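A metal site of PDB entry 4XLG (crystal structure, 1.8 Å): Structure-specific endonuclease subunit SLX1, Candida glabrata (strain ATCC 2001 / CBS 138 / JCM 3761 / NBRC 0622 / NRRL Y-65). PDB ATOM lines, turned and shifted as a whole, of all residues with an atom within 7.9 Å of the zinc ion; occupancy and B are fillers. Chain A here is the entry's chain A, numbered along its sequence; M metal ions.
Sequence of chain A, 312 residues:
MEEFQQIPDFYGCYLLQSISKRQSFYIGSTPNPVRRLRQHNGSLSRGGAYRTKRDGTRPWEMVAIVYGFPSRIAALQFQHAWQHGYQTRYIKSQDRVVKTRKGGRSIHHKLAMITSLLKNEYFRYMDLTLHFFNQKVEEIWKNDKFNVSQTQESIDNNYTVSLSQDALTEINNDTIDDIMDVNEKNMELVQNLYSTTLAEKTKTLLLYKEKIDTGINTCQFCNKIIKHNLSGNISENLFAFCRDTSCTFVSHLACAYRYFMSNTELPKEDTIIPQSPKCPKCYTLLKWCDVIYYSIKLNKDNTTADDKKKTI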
ATOM      1  N   THR A 218     -15.354  20.256   1.295  1.00  0.00           N
ATOM      2  CA  THR A 218     -14.020  19.899   0.798  1.00  0.00           C
ATOM      3  C   THR A 218     -13.721  18.446   1.127  1.00  0.00           C
ATOM      4  O   THR A 218     -14.335  17.861   2.036  1.00  0.00           O
ATOM      5  CB  THR A 218     -12.923  20.780   1.400  1.00  0.00           C
ATOM      6  OG1 THR A 218     -13.009  20.723   2.823  1.00  0.00           O
ATOM      7  CG2 THR A 218     -13.051  22.227   0.926  1.00  0.00           C
ATOM      8  N   CYS A 219     -12.779  17.855   0.394  1.00  0.00           N
ATOM      9  CA  CYS A 219     -12.534  16.416   0.530  1.00  0.00           C
ATOM     10  C   CYS A 219     -11.780  16.183   1.842  1.00  0.00           C
ATOM     11  O   CYS A 219     -10.765  16.835   2.111  1.00  0.00           O
ATOM     12  CB  CYS A 219     -11.746  15.863  -0.659  1.00  0.00           C
ATOM     13  SG  CYS A 219     -10.970  14.225  -0.390  1.00  0.00           S
ATOM     14  N   GLN A 220     -12.297  15.273   2.658  1.00  0.00           N
ATOM     15  CA  GLN A 220     -11.661  14.936   3.930  1.00  0.00           C
ATOM     16  C   GLN A 220     -10.140  14.746   3.812  1.00  0.00           C
ATOM     17  O   GLN A 220      -9.406  15.137   4.706  1.00  0.00           O
ATOM     18  CB  GLN A 220     -12.289  13.678   4.529  1.00  0.00           C
ATOM     19  CG  GLN A 220     -11.545  13.127   5.762  1.00  0.00           C
ATOM     20  CD  GLN A 220     -11.907  13.834   7.066  1.00  0.00           C
ATOM     21  OE1 GLN A 220     -12.886  14.577   7.141  1.00  0.00           O
ATOM     22  NE2 GLN A 220     -11.116  13.595   8.092  1.00  0.00           N
ATOM     23  N   PHE A 221      -9.675  14.150   2.702  1.00  0.00           N
ATOM     24  CA  PHE A 221      -8.259  13.790   2.536  1.00  0.00           C
ATOM     25  C   PHE A 221      -7.434  14.742   1.671  1.00  0.00           C
ATOM     26  O   PHE A 221      -6.349  15.132   2.078  1.00  0.00           O
ATOM     27  CB  PHE A 221      -8.155  12.366   1.971  1.00  0.00           C
ATOM     28  CG  PHE A 221      -9.022  11.398   2.683  1.00  0.00           C
ATOM     29  CD1 PHE A 221      -8.632  10.862   3.908  1.00  0.00           C
ATOM     30  CD2 PHE A 221     -10.257  11.073   2.174  1.00  0.00           C
ATOM     31  CE1 PHE A 221      -9.475  10.002   4.595  1.00  0.00           C
ATOM     32  CE2 PHE A 221     -11.107  10.188   2.847  1.00  0.00           C
ATOM     33  CZ  PHE A 221     -10.716   9.657   4.056  1.00  0.00           C
ATOM     34  N   CYS A 222      -7.926  15.139   0.499  1.00  0.00           N
ATOM     35  CA  CYS A 222      -7.094  15.971  -0.380  1.00  0.00           C
ATOM     36  C   CYS A 222      -7.463  17.455  -0.314  1.00  0.00           C
ATOM     37  O   CYS A 222      -6.753  18.306  -0.871  1.00  0.00           O
ATOM     38  CB  CYS A 222      -7.199  15.490  -1.830  1.00  0.00           C
ATOM     39  SG  CYS A 222      -8.691  16.067  -2.685  1.00  0.00           S
ATOM     40  N   ASN A 223      -8.579  17.768   0.356  1.00  0.00           N
ATOM     41  CA  ASN A 223      -8.988  19.162   0.671  1.00  0.00           C
ATOM     42  C   ASN A 223      -9.550  19.979  -0.503  1.00  0.00           C
ATOM     43  O   ASN A 223      -9.903  21.150  -0.331  1.00  0.00           O
ATOM     44  CB  ASN A 223      -7.814  19.950   1.284  1.00  0.00           C
ATOM     45  CG  ASN A 223      -7.336  19.343   2.588  1.00  0.00           C
ATOM     46  OD1 ASN A 223      -8.120  19.167   3.524  1.00  0.00           O
ATOM     47  ND2 ASN A 223      -6.051  18.996   2.656  1.00  0.00           N
ATOM     48  N   LYS A 224      -9.633  19.401  -1.691  1.00  0.00           N
ATOM     49  CA  LYS A 224     -10.184  20.150  -2.813  1.00  0.00           C
ATOM     50  C   LYS A 224     -11.691  20.207  -2.683  1.00  0.00           C
ATOM     51  O   LYS A 224     -12.311  19.315  -2.087  1.00  0.00           O
ATOM     52  CB  LYS A 224      -9.800  19.522  -4.133  1.00  0.00           C
ATOM     53  CG  LYS A 224      -8.314  19.526  -4.402  1.00  0.00           C
ATOM     54  CD  LYS A 224      -8.042  18.661  -5.616  1.00  0.00           C
ATOM     55  CE  LYS A 224      -6.568  18.578  -5.932  1.00  0.00           C
ATOM     56  NZ  LYS A 224      -6.383  17.553  -6.989  1.00  0.00           N
ATOM     57  N   ILE A 225     -12.284  21.270  -3.239  1.00  0.00           N
ATOM     58  CA  ILE A 225     -13.725  21.478  -3.160  1.00  0.00           C
ATOM     59  C   ILE A 225     -14.525  20.338  -3.770  1.00  0.00           C
ATOM     60  O   ILE A 225     -14.196  19.828  -4.848  1.00  0.00           O
ATOM     61  CB  ILE A 225     -14.134  22.816  -3.829  1.00  0.00           C
ATOM     62  CG1 ILE A 225     -13.592  23.989  -3.027  1.00  0.00           C
ATOM     63  CG2 ILE A 225     -15.643  22.920  -3.952  1.00  0.00           C
ATOM     64  CD1 ILE A 225     -14.302  24.193  -1.709  1.00  0.00           C
ATOM     65  N   ILE A 226     -15.567  19.916  -3.067  1.00  0.00           N
ATOM     66  CA  ILE A 226     -16.505  18.936  -3.608  1.00  0.00           C
ATOM     67  C   ILE A 226     -17.487  19.596  -4.605  1.00  0.00           C
ATOM     68  O   ILE A 226     -18.326  20.426  -4.209  1.00  0.00           O
ATOM     69  CB  ILE A 226     -17.285  18.234  -2.478  1.00  0.00           C
ATOM     70  CG1 ILE A 226     -16.311  17.609  -1.470  1.00  0.00           C
ATOM     71  CG2 ILE A 226     -18.235  17.185  -3.072  1.00  0.00           C
ATOM     72  CD1 ILE A 226     -15.579  16.345  -1.987  1.00  0.00           C
ATOM     73  N   SER A 235     -12.678   9.897 -11.642  1.00  0.00           N
ATOM     74  CA  SER A 235     -12.036   9.999 -10.336  1.00  0.00           C
ATOM     75  C   SER A 235     -12.379  11.309  -9.650  1.00  0.00           C
ATOM     76  O   SER A 235     -12.321  11.421  -8.414  1.00  0.00           O
ATOM     77  CB  SER A 235     -10.501   9.861 -10.454  1.00  0.00           C
ATOM     78  OG  SER A 235      -9.907  11.103 -10.806  1.00  0.00           O
ATOM     79  N   LEU A 238     -16.782  11.071  -8.549  1.00  0.00           N
ATOM     80  CA  LEU A 238     -17.346  10.069  -7.663  1.00  0.00           C
ATOM     81  C   LEU A 238     -17.014  10.481  -6.225  1.00  0.00           C
ATOM     82  O   LEU A 238     -15.841  10.680  -5.887  1.00  0.00           O
ATOM     83  CB  LEU A 238     -16.802   8.673  -7.977  1.00  0.00           C
ATOM     84  CG  LEU A 238     -17.240   8.030  -9.289  1.00  0.00           C
ATOM     85  CD1 LEU A 238     -16.658   6.585  -9.387  1.00  0.00           C
ATOM     86  CD2 LEU A 238     -18.787   8.022  -9.371  1.00  0.00           C
ATOM     87  N   PHE A 239     -18.047  10.620  -5.400  1.00  0.00           N
ATOM     88  CA  PHE A 239     -17.888  11.074  -4.036  1.00  0.00           C
ATOM     89  C   PHE A 239     -18.293   9.991  -3.064  1.00  0.00           C
ATOM     90  O   PHE A 239     -19.020   9.064  -3.426  1.00  0.00           O
ATOM     91  CB  PHE A 239     -18.712  12.308  -3.788  1.00  0.00           C
ATOM     92  CG  PHE A 239     -18.420  13.415  -4.758  1.00  0.00           C
ATOM     93  CD1 PHE A 239     -17.148  13.967  -4.830  1.00  0.00           C
ATOM     94  CD2 PHE A 239     -19.395  13.876  -5.618  1.00  0.00           C
ATOM     95  CE1 PHE A 239     -16.852  14.998  -5.739  1.00  0.00           C
ATOM     96  CE2 PHE A 239     -19.128  14.912  -6.515  1.00  0.00           C
ATOM     97  CZ  PHE A 239     -17.841  15.473  -6.589  1.00  0.00           C
ATOM     98  N   VAL A 250     -17.255  13.898   4.043  1.00  0.00           N
ATOM     99  CA  VAL A 250     -17.423  13.786   2.601  1.00  0.00           C
ATOM    100  C   VAL A 250     -16.025  13.741   1.965  1.00  0.00           C
ATOM    101  O   VAL A 250     -15.120  14.409   2.446  1.00  0.00           O
ATOM    102  CB  VAL A 250     -18.270  14.954   2.030  1.00  0.00           C
ATOM    103  CG1 VAL A 250     -17.647  16.305   2.365  1.00  0.00           C
ATOM    104  CG2 VAL A 250     -18.514  14.799   0.546  1.00  0.00           C
ATOM    105  N   SER A 251     -15.833  12.940   0.920  1.00  0.00           N
ATOM    106  CA  SER A 251     -14.538  12.890   0.228  1.00  0.00           C
ATOM    107  C   SER A 251     -14.725  12.513  -1.258  1.00  0.00           C
ATOM    108  O   SER A 251     -15.817  12.121  -1.671  1.00  0.00           O
ATOM    109  CB  SER A 251     -13.618  11.838   0.907  1.00  0.00           C
ATOM    110  OG  SER A 251     -14.139  10.543   0.656  1.00  0.00           O
ATOM    111  N   HIS A 252     -13.660  12.619  -2.032  1.00  0.00           N
ATOM    112  CA  HIS A 252     -13.596  11.912  -3.320  1.00  0.00           C
ATOM    113  C   HIS A 252     -13.634  10.437  -3.046  1.00  0.00           C
ATOM    114  O   HIS A 252     -12.989   9.987  -2.102  1.00  0.00           O
ATOM    115  CB  HIS A 252     -12.311  12.312  -4.079  1.00  0.00           C
ATOM    116  CG  HIS A 252     -12.322  13.751  -4.507  1.00  0.00           C
ATOM    117  ND1 HIS A 252     -11.415  14.674  -4.047  1.00  0.00           N
ATOM    118  CD2 HIS A 252     -13.172  14.427  -5.310  1.00  0.00           C
ATOM    119  CE1 HIS A 252     -11.699  15.863  -4.551  1.00  0.00           C
ATOM    120  NE2 HIS A 252     -12.772  15.738  -5.315  1.00  0.00           N
ATOM    121  N   LEU A 253     -14.352   9.659  -3.870  1.00  0.00           N
ATOM    122  CA  LEU A 253     -14.348   8.215  -3.729  1.00  0.00           C
ATOM    123  C   LEU A 253     -12.915   7.651  -3.808  1.00  0.00           C
ATOM    124  O   LEU A 253     -12.526   6.775  -3.002  1.00  0.00           O
ATOM    125  CB  LEU A 253     -15.209   7.540  -4.799  1.00  0.00           C
ATOM    126  CG  LEU A 253     -15.383   6.018  -4.651  1.00  0.00           C
ATOM    127  CD1 LEU A 253     -16.025   5.626  -3.292  1.00  0.00           C
ATOM    128  CD2 LEU A 253     -16.188   5.425  -5.826  1.00  0.00           C
ATOM    129  N   ALA A 254     -12.143   8.131  -4.780  1.00  0.00           N
ATOM    130  CA  ALA A 254     -10.757   7.656  -4.911  1.00  0.00           C
ATOM    131  C   ALA A 254      -9.948   7.947  -3.664  1.00  0.00           C
ATOM    132  O   ALA A 254      -9.114   7.127  -3.254  1.00  0.00           O
ATOM    133  CB  ALA A 254     -10.064   8.279  -6.132  1.00  0.00           C
ATOM    134  N   CYS A 255     -10.159   9.119  -3.077  1.00  0.00           N
ATOM    135  CA  CYS A 255      -9.433   9.492  -1.874  1.00  0.00           C
ATOM    136  C   CYS A 255      -9.807   8.603  -0.680  1.00  0.00           C
ATOM    137  O   CYS A 255      -8.941   8.206   0.111  1.00  0.00           O
ATOM    138  CB  CYS A 255      -9.666  10.968  -1.554  1.00  0.00           C
ATOM    139  SG  CYS A 255      -8.883  11.995  -2.852  1.00  0.00           S
ATOM    140  N   ALA A 256     -11.103   8.315  -0.536  1.00  0.00           N
ATOM    141  CA  ALA A 256     -11.563   7.466   0.545  1.00  0.00           C
ATOM    142  C   ALA A 256     -10.997   6.061   0.338  1.00  0.00           C
ATOM    143  O   ALA A 256     -10.464   5.441   1.271  1.00  0.00           O
ATOM    144  CB  ALA A 256     -13.088   7.434   0.591  1.00  0.00           C
HETATM  145 ZN    ZN M   1      -9.996  14.110  -2.449  1.00  0.00          ZN
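The backbone NH of Phe 221 lies close to the side-chain sulfur of Cys 219, 3.4 Å away. The backbone NH (N) of Cys 219 lies within hydrogen-bond range of the backbone carbonyl oxygen (O) of Lys 224, 2.9 Å away. N of Lys 224 lies close to SG of Cys 222 (3.6 Å).
Four residues have an atom within 4 Å of the zinc ion: Cys 219, Cys 222, His 252 and Cys 255. The nearest printed residue that does not touch the zinc ion is Asn 223 (4.8 Å).
The zinc ion is bound by a ring nitrogen (ND1) of His 252 (2.2 Å), the side-chain sulfur (SG) of Cys 219 (2.3 Å), the side-chain sulfur (SG) of Cys 222 (2.4 Å) and the side-chain sulfur (SG) of Cys 255 (2.4 Å).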
